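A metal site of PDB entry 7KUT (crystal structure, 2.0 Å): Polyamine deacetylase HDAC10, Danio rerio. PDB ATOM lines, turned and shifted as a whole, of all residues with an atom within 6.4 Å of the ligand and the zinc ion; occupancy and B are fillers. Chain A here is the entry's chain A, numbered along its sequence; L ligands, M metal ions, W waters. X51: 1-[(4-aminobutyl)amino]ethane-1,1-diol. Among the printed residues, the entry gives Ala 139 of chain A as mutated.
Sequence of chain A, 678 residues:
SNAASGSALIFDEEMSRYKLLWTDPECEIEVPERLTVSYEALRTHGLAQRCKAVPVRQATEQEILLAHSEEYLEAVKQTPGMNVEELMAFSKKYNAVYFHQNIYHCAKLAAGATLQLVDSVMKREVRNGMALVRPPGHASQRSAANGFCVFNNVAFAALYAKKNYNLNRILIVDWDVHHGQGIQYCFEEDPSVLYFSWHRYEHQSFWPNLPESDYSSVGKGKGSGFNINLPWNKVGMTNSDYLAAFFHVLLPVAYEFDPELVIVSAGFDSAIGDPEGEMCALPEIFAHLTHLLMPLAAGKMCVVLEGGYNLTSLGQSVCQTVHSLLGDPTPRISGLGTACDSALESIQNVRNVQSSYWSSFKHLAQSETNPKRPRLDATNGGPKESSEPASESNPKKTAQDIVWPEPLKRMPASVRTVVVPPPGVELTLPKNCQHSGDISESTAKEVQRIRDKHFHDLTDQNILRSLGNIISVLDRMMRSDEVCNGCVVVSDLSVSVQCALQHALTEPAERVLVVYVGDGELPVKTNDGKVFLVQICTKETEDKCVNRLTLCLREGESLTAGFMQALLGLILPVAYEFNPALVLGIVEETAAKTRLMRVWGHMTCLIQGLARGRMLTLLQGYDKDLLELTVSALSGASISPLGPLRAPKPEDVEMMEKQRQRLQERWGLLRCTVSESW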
ATOM      1  N   GLU A  26       7.541   3.992 -27.036  1.00  0.00           N
ATOM      2  CA  GLU A  26       7.280   5.410 -27.212  1.00  0.00           C
ATOM      3  C   GLU A  26       5.831   5.681 -27.603  1.00  0.00           C
ATOM      4  O   GLU A  26       5.220   6.630 -27.100  1.00  0.00           O
ATOM      5  CB  GLU A  26       8.231   5.975 -28.275  1.00  0.00           C
ATOM      6  CG  GLU A  26       9.208   6.982 -27.756  1.00  0.00           C
ATOM      7  CD  GLU A  26       9.715   7.903 -28.842  1.00  0.00           C
ATOM      8  OE1 GLU A  26      10.230   7.393 -29.866  1.00  0.00           O
ATOM      9  OE2 GLU A  26       9.589   9.135 -28.670  1.00  0.00           O
ATOM     10  N   CYS A  27       5.252   4.870 -28.504  1.00  0.00           N
ATOM     11  CA  CYS A  27       3.920   5.163 -29.032  1.00  0.00           C
ATOM     12  C   CYS A  27       2.809   4.286 -28.465  1.00  0.00           C
ATOM     13  O   CYS A  27       1.635   4.567 -28.735  1.00  0.00           O
ATOM     14  CB  CYS A  27       3.890   5.035 -30.560  1.00  0.00           C
ATOM     15  SG  CYS A  27       5.110   6.003 -31.463  1.00  0.00           S
ATOM     16  N   ILE A  29       1.261   4.240 -25.841  1.00  0.00           N
ATOM     17  CA  ILE A  29       0.248   4.922 -25.030  1.00  0.00           C
ATOM     18  C   ILE A  29      -0.890   5.488 -25.865  1.00  0.00           C
ATOM     19  O   ILE A  29      -1.966   5.783 -25.320  1.00  0.00           O
ATOM     20  CB  ILE A  29       0.834   6.106 -24.236  1.00  0.00           C
ATOM     21  CG1 ILE A  29       1.544   7.058 -25.204  1.00  0.00           C
ATOM     22  CG2 ILE A  29       1.741   5.620 -23.133  1.00  0.00           C
ATOM     23  CD1 ILE A  29       1.995   8.364 -24.563  1.00  0.00           C
ATOM     24  N   ASN A  95       9.473  11.203 -36.053  1.00  0.00           N
ATOM     25  CA  ASN A  95       9.742  11.116 -34.623  1.00  0.00           C
ATOM     26  C   ASN A  95       8.456  10.875 -33.836  1.00  0.00           C
ATOM     27  O   ASN A  95       7.534  11.705 -33.873  1.00  0.00           O
ATOM     28  CB  ASN A  95      10.435  12.383 -34.134  1.00  0.00           C
ATOM     29  CG  ASN A  95      11.827  12.538 -34.710  1.00  0.00           C
ATOM     30  OD1 ASN A  95      12.560  11.567 -34.852  1.00  0.00           O
ATOM     31  ND2 ASN A  95      12.183  13.764 -35.060  1.00  0.00           N
ATOM     32  N   ALA A  96       8.398   9.748 -33.124  1.00  0.00           N
ATOM     33  CA  ALA A  96       7.302   9.419 -32.205  1.00  0.00           C
ATOM     34  C   ALA A  96       5.943   9.358 -32.909  1.00  0.00           C
ATOM     35  O   ALA A  96       4.968  10.003 -32.504  1.00  0.00           O
ATOM     36  CB  ALA A  96       7.272  10.406 -31.022  1.00  0.00           C
ATOM     37  N   PRO A 136      -4.276  12.932 -33.154  1.00  0.00           N
ATOM     38  CA  PRO A 136      -4.139  14.341 -32.752  1.00  0.00           C
ATOM     39  C   PRO A 136      -3.351  15.102 -33.809  1.00  0.00           C
ATOM     40  O   PRO A 136      -2.870  14.541 -34.797  1.00  0.00           O
ATOM     41  CB  PRO A 136      -3.400  14.275 -31.419  1.00  0.00           C
ATOM     42  CG  PRO A 136      -2.608  12.995 -31.477  1.00  0.00           C
ATOM     43  CD  PRO A 136      -3.481  12.034 -32.295  1.00  0.00           C
ATOM     44  N   GLY A 137      -3.267  16.421 -33.627  1.00  0.00           N
ATOM     45  CA  GLY A 137      -2.687  17.219 -34.701  1.00  0.00           C
ATOM     46  C   GLY A 137      -1.578  18.210 -34.382  1.00  0.00           C
ATOM     47  O   GLY A 137      -0.742  18.476 -35.250  1.00  0.00           O
ATOM     48  N   HIS A 138      -1.511  18.738 -33.138  1.00  0.00           N
ATOM     49  CA  HIS A 138      -0.778  19.994 -32.914  1.00  0.00           C
ATOM     50  C   HIS A 138       0.738  19.865 -33.124  1.00  0.00           C
ATOM     51  O   HIS A 138       1.404  20.884 -33.355  1.00  0.00           O
ATOM     52  CB  HIS A 138      -1.103  20.580 -31.516  1.00  0.00           C
ATOM     53  CG  HIS A 138      -0.494  19.836 -30.366  1.00  0.00           C
ATOM     54  ND1 HIS A 138      -0.192  20.465 -29.167  1.00  0.00           N
ATOM     55  CD2 HIS A 138      -0.158  18.535 -30.204  1.00  0.00           C
ATOM     56  CE1 HIS A 138       0.314  19.580 -28.324  1.00  0.00           C
ATOM     57  NE2 HIS A 138       0.348  18.401 -28.929  1.00  0.00           N
ATOM     58  N   ALA A 139       1.283  18.655 -33.113  1.00  0.00           N
ATOM     59  CA  ALA A 139       2.704  18.480 -33.373  1.00  0.00           C
ATOM     60  C   ALA A 139       3.052  18.269 -34.840  1.00  0.00           C
ATOM     61  O   ALA A 139       4.241  18.352 -35.187  1.00  0.00           O
ATOM     62  CB  ALA A 139       3.252  17.280 -32.581  1.00  0.00           C
ATOM     63  N   ASN A 146       4.568  13.852 -36.619  1.00  0.00           N
ATOM     64  CA  ASN A 146       5.362  14.025 -35.411  1.00  0.00           C
ATOM     65  C   ASN A 146       4.473  13.823 -34.192  1.00  0.00           C
ATOM     66  O   ASN A 146       3.353  14.335 -34.151  1.00  0.00           O
ATOM     67  CB  ASN A 146       6.005  15.414 -35.386  1.00  0.00           C
ATOM     68  CG  ASN A 146       6.985  15.585 -34.261  1.00  0.00           C
ATOM     69  OD1 ASN A 146       6.620  16.059 -33.188  1.00  0.00           O
ATOM     70  ND2 ASN A 146       8.235  15.215 -34.496  1.00  0.00           N
ATOM     71  N   GLY A 147       4.984  13.086 -33.214  1.00  0.00           N
ATOM     72  CA  GLY A 147       4.318  12.992 -31.925  1.00  0.00           C
ATOM     73  C   GLY A 147       2.878  12.517 -31.997  1.00  0.00           C
ATOM     74  O   GLY A 147       1.982  13.182 -31.466  1.00  0.00           O
ATOM     75  N   PHE A 148       2.655  11.381 -32.657  1.00  0.00           N
ATOM     76  CA  PHE A 148       1.358  10.754 -32.908  1.00  0.00           C
ATOM     77  C   PHE A 148       0.467  11.563 -33.832  1.00  0.00           C
ATOM     78  O   PHE A 148      -0.668  11.142 -34.089  1.00  0.00           O
ATOM     79  CB  PHE A 148       0.546  10.472 -31.627  1.00  0.00           C
ATOM     80  CG  PHE A 148       1.357   9.985 -30.452  1.00  0.00           C
ATOM     81  CD1 PHE A 148       2.411   9.110 -30.640  1.00  0.00           C
ATOM     82  CD2 PHE A 148       1.025  10.364 -29.153  1.00  0.00           C
ATOM     83  CE1 PHE A 148       3.155   8.656 -29.549  1.00  0.00           C
ATOM     84  CE2 PHE A 148       1.750   9.892 -28.082  1.00  0.00           C
ATOM     85  CZ  PHE A 148       2.813   9.041 -28.285  1.00  0.00           C
ATOM     86  N   CYS A 149       0.935  12.702 -34.354  1.00  0.00           N
ATOM     87  CA  CYS A 149       0.130  13.569 -35.210  1.00  0.00           C
ATOM     88  C   CYS A 149       0.480  13.410 -36.691  1.00  0.00           C
ATOM     89  O   CYS A 149       1.661  13.369 -37.054  1.00  0.00           O
ATOM     90  CB  CYS A 149       0.297  15.027 -34.791  1.00  0.00           C
ATOM     91  SG  CYS A 149      -0.042  15.360 -33.041  1.00  0.00           S
ATOM     92  N   ASP A 176      -2.648  21.112 -23.954  1.00  0.00           N
ATOM     93  CA  ASP A 176      -1.920  19.854 -23.958  1.00  0.00           C
ATOM     94  C   ASP A 176      -0.596  20.051 -23.231  1.00  0.00           C
ATOM     95  O   ASP A 176      -0.058  21.157 -23.188  1.00  0.00           O
ATOM     96  CB  ASP A 176      -1.686  19.417 -25.415  1.00  0.00           C
ATOM     97  CG  ASP A 176      -1.172  18.002 -25.544  1.00  0.00           C
ATOM     98  OD1 ASP A 176      -1.978  17.111 -25.883  1.00  0.00           O
ATOM     99  OD2 ASP A 176       0.041  17.761 -25.319  1.00  0.00           O
ATOM    100  N   VAL A 177      -0.082  18.981 -22.619  1.00  0.00           N
ATOM    101  CA  VAL A 177       1.141  19.098 -21.830  1.00  0.00           C
ATOM    102  C   VAL A 177       2.392  19.168 -22.700  1.00  0.00           C
ATOM    103  O   VAL A 177       3.489  19.441 -22.184  1.00  0.00           O
ATOM    104  CB  VAL A 177       1.263  17.933 -20.823  1.00  0.00           C
ATOM    105  CG1 VAL A 177       1.917  16.703 -21.479  1.00  0.00           C
ATOM    106  CG2 VAL A 177       2.010  18.383 -19.549  1.00  0.00           C
ATOM    107  N   HIS A 178       2.262  18.918 -24.000  1.00  0.00           N
ATOM    108  CA  HIS A 178       3.352  19.030 -24.955  1.00  0.00           C
ATOM    109  C   HIS A 178       3.188  20.330 -25.738  1.00  0.00           C
ATOM    110  O   HIS A 178       2.072  20.794 -25.968  1.00  0.00           O
ATOM    111  CB  HIS A 178       3.366  17.838 -25.931  1.00  0.00           C
ATOM    112  CG  HIS A 178       3.566  16.506 -25.266  1.00  0.00           C
ATOM    113  ND1 HIS A 178       2.525  15.680 -24.914  1.00  0.00           N
ATOM    114  CD2 HIS A 178       4.696  15.832 -24.947  1.00  0.00           C
ATOM    115  CE1 HIS A 178       2.995  14.567 -24.386  1.00  0.00           C
ATOM    116  NE2 HIS A 178       4.313  14.629 -24.390  1.00  0.00           N
ATOM    117  N   HIS A 179       4.321  20.910 -26.148  1.00  0.00           N
ATOM    118  CA  HIS A 179       4.296  22.055 -27.058  1.00  0.00           C
ATOM    119  C   HIS A 179       3.664  21.652 -28.393  1.00  0.00           C
ATOM    120  O   HIS A 179       3.943  20.579 -28.931  1.00  0.00           O
ATOM    121  CB  HIS A 179       5.718  22.558 -27.298  1.00  0.00           C
ATOM    122  CG  HIS A 179       5.794  23.862 -28.028  1.00  0.00           C
ATOM    123  ND1 HIS A 179       6.764  24.130 -28.966  1.00  0.00           N
ATOM    124  CD2 HIS A 179       5.037  24.975 -27.933  1.00  0.00           C
ATOM    125  CE1 HIS A 179       6.585  25.352 -29.443  1.00  0.00           C
ATOM    126  NE2 HIS A 179       5.544  25.882 -28.829  1.00  0.00           N
ATOM    127  N   TRP A 207      10.405  16.064 -24.362  1.00  0.00           N
ATOM    128  CA  TRP A 207       9.889  16.025 -25.724  1.00  0.00           C
ATOM    129  C   TRP A 207       8.964  17.216 -26.000  1.00  0.00           C
ATOM    130  O   TRP A 207       8.096  17.523 -25.177  1.00  0.00           O
ATOM    131  CB  TRP A 207       9.154  14.697 -25.946  1.00  0.00           C
ATOM    132  CG  TRP A 207       8.970  14.404 -27.387  1.00  0.00           C
ATOM    133  CD1 TRP A 207       9.799  13.692 -28.203  1.00  0.00           C
ATOM    134  CD2 TRP A 207       7.915  14.894 -28.222  1.00  0.00           C
ATOM    135  NE1 TRP A 207       9.317  13.694 -29.495  1.00  0.00           N
ATOM    136  CE2 TRP A 207       8.166  14.433 -29.527  1.00  0.00           C
ATOM    137  CE3 TRP A 207       6.789  15.687 -27.983  1.00  0.00           C
ATOM    138  CZ2 TRP A 207       7.314  14.712 -30.589  1.00  0.00           C
ATOM    139  CZ3 TRP A 207       5.943  15.974 -29.043  1.00  0.00           C
ATOM    140  CH2 TRP A 207       6.208  15.487 -30.334  1.00  0.00           C
ATOM    141  N   GLY A 267      -5.420  18.973 -24.999  1.00  0.00           N
ATOM    142  CA  GLY A 267      -4.789  17.758 -24.542  1.00  0.00           C
ATOM    143  C   GLY A 267      -4.948  17.646 -23.042  1.00  0.00           C
ATOM    144  O   GLY A 267      -4.616  18.578 -22.302  1.00  0.00           O
ATOM    145  N   ASP A 269      -3.475  15.277 -21.332  1.00  0.00           N
ATOM    146  CA  ASP A 269      -2.275  14.773 -20.692  1.00  0.00           C
ATOM    147  C   ASP A 269      -1.650  15.802 -19.762  1.00  0.00           C
ATOM    148  O   ASP A 269      -0.610  15.534 -19.164  1.00  0.00           O
ATOM    149  CB  ASP A 269      -1.258  14.288 -21.737  1.00  0.00           C
ATOM    150  CG  ASP A 269      -0.957  15.319 -22.842  1.00  0.00           C
ATOM    151  OD1 ASP A 269      -1.339  16.508 -22.723  1.00  0.00           O
ATOM    152  OD2 ASP A 269      -0.304  14.895 -23.828  1.00  0.00           O
ATOM    153  N   GLU A 276       2.607  10.778 -19.372  1.00  0.00           N
ATOM    154  CA  GLU A 276       3.477  11.697 -20.094  1.00  0.00           C
ATOM    155  C   GLU A 276       3.643  13.022 -19.381  1.00  0.00           C
ATOM    156  O   GLU A 276       4.763  13.546 -19.300  1.00  0.00           O
ATOM    157  CB  GLU A 276       2.920  11.955 -21.502  1.00  0.00           C
ATOM    158  CG  GLU A 276       3.270  10.905 -22.504  1.00  0.00           C
ATOM    159  CD  GLU A 276       4.739  10.938 -22.852  1.00  0.00           C
ATOM    160  OE1 GLU A 276       5.177  11.903 -23.532  1.00  0.00           O
ATOM    161  OE2 GLU A 276       5.454   9.995 -22.453  1.00  0.00           O
ATOM    162  N   GLU A 306      -6.593  16.729 -28.377  1.00  0.00           N
ATOM    163  CA  GLU A 306      -5.226  16.380 -28.749  1.00  0.00           C
ATOM    164  C   GLU A 306      -4.806  15.140 -27.965  1.00  0.00           C
ATOM    165  O   GLU A 306      -5.271  14.029 -28.281  1.00  0.00           O
ATOM    166  CB  GLU A 306      -4.286  17.585 -28.542  1.00  0.00           C
ATOM    167  CG  GLU A 306      -4.747  18.809 -29.311  1.00  0.00           C
ATOM    168  CD  GLU A 306      -4.151  18.893 -30.733  1.00  0.00           C
ATOM    169  OE1 GLU A 306      -3.462  17.938 -31.177  1.00  0.00           O
ATOM    170  OE2 GLU A 306      -4.344  19.931 -31.405  1.00  0.00           O
ATOM    171  N   GLY A 307      -3.930  15.258 -26.968  1.00  0.00           N
ATOM    172  CA  GLY A 307      -3.458  14.116 -26.207  1.00  0.00           C
ATOM    173  C   GLY A 307      -4.289  13.830 -24.955  1.00  0.00           C
ATOM    174  O   GLY A 307      -5.385  14.364 -24.765  1.00  0.00           O
ATOM    175  N   GLY A 308      -3.748  12.945 -24.100  1.00  0.00           N
ATOM    176  CA  GLY A 308      -4.385  12.526 -22.846  1.00  0.00           C
ATOM    177  C   GLY A 308      -4.428  11.017 -22.713  1.00  0.00           C
ATOM    178  O   GLY A 308      -5.182  10.366 -23.435  1.00  0.00           O
ATOM    179  N   TYR A 309      -3.603  10.435 -21.831  1.00  0.00           N
ATOM    180  CA  TYR A 309      -3.270   9.020 -21.949  1.00  0.00           C
ATOM    181  C   TYR A 309      -3.610   8.171 -20.732  1.00  0.00           C
ATOM    182  O   TYR A 309      -3.474   6.953 -20.814  1.00  0.00           O
ATOM    183  CB  TYR A 309      -1.768   8.841 -22.277  1.00  0.00           C
ATOM    184  CG  TYR A 309      -1.435   9.644 -23.492  1.00  0.00           C
ATOM    185  CD1 TYR A 309      -1.778   9.183 -24.751  1.00  0.00           C
ATOM    186  CD2 TYR A 309      -0.845  10.904 -23.381  1.00  0.00           C
ATOM    187  CE1 TYR A 309      -1.523   9.945 -25.880  1.00  0.00           C
ATOM    188  CE2 TYR A 309      -0.568  11.655 -24.482  1.00  0.00           C
ATOM    189  CZ  TYR A 309      -0.908  11.180 -25.742  1.00  0.00           C
ATOM    190  OH  TYR A 309      -0.652  11.934 -26.851  1.00  0.00           O
HETATM  191  C01 X51 L   1      -0.478  14.787 -28.980  1.00  0.00           C
HETATM  192  C02 X51 L   1       0.714  14.862 -28.004  1.00  0.00           C
HETATM  193  C06 X51 L   1       2.562  13.294 -27.621  1.00  0.00           C
HETATM  194  C07 X51 L   1       3.923  12.857 -28.197  1.00  0.00           C
HETATM  195  C08 X51 L   1       4.688  11.963 -27.220  1.00  0.00           C
HETATM  196  C09 X51 L   1       6.101  11.614 -27.715  1.00  0.00           C
HETATM  197  N05 X51 L   1       1.857  14.142 -28.570  1.00  0.00           N
HETATM  198  N10 X51 L   1       6.724  10.671 -26.805  1.00  0.00           N
HETATM  199  O03 X51 L   1       1.095  16.193 -27.864  1.00  0.00           O
HETATM  200  O04 X51 L   1       0.276  14.355 -26.784  1.00  0.00           O
HETATM  201 ZN    ZN M   1       0.421  15.949 -25.399  1.00  0.00          ZN
HETATM  202  O   HOH W   1       5.423   8.393 -24.812  1.00  0.00           O
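Residues that only touch the ligand: Ala 96 (3.7 Å), Pro 136 (3.7 Å), Phe 148 (3.5 Å), Trp 207 (3.8 Å) and Gly 307 (3.8 Å).
NE2 of His 178 sits at hydrogen-bond distance from OE1 of Glu 276 (3.0 Å).
O of Gly 147 sits at hydrogen-bond distance from SG of Cys 149, at 3.4 Å.
O of Ala 96 sits close to N of Gly 147 (3.2 Å).
The backbone carbonyl oxygen (O) of Asn 95 lies within hydrogen-bond range of the backbone NH (N) of Gly 147 (3.0 Å).
OD1 of Asp 269 lies within hydrogen-bond range of N of Val 177 (2.8 Å).
N of His 138 sits at hydrogen-bond distance from OE1 of Glu 306, 2.9 Å away.
N of Phe 148 sits at hydrogen-bond distance from O of Ala 96, 2.7 Å away.
N of Gly 307 lies within hydrogen-bond range of OD1 of Asp 176 (2.9 Å).
The zinc ion is bound by OD2 of Asp 176 (1.9 Å), OD2 of Asp 269 (2.0 Å), O04 of the ligand (2.1 Å), ND1 of His 178 (2.2 Å) and O03 of the ligand (2.6 Å).
The zinc ion has five donor atoms within binding distance.
Slightly farther from the zinc ion lies the side-chain carboxylate (OD1) of Asp 176 (2.7 Å).
A nitrogen (N05) of the ligand is in hydrogen-bond range of the backbone carbonyl oxygen of Gly 147, at 3.1 Å.
NE2 of His 138 lies close to O03 of the ligand, at 2.6 Å.
A nitrogen (N10) of the ligand lies within salt-bridge range of the side-chain carboxylate of Glu 276 (3.8 Å).
The side-chain carboxylate (OE2) of Glu 26 lies within salt-bridge range of a nitrogen (N10) of the ligand (3.7 Å).
An oxygen (O04) of the ligand lies close to the side-chain hydroxyl of Tyr 309 (2.6 Å).
Of the 25 residues printed, 3 come within 4 Å of the zinc ion.
Water W1 lies within hydrogen-bond range of OE2 of Glu 276, O of Glu 26 and N10 of the ligand.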
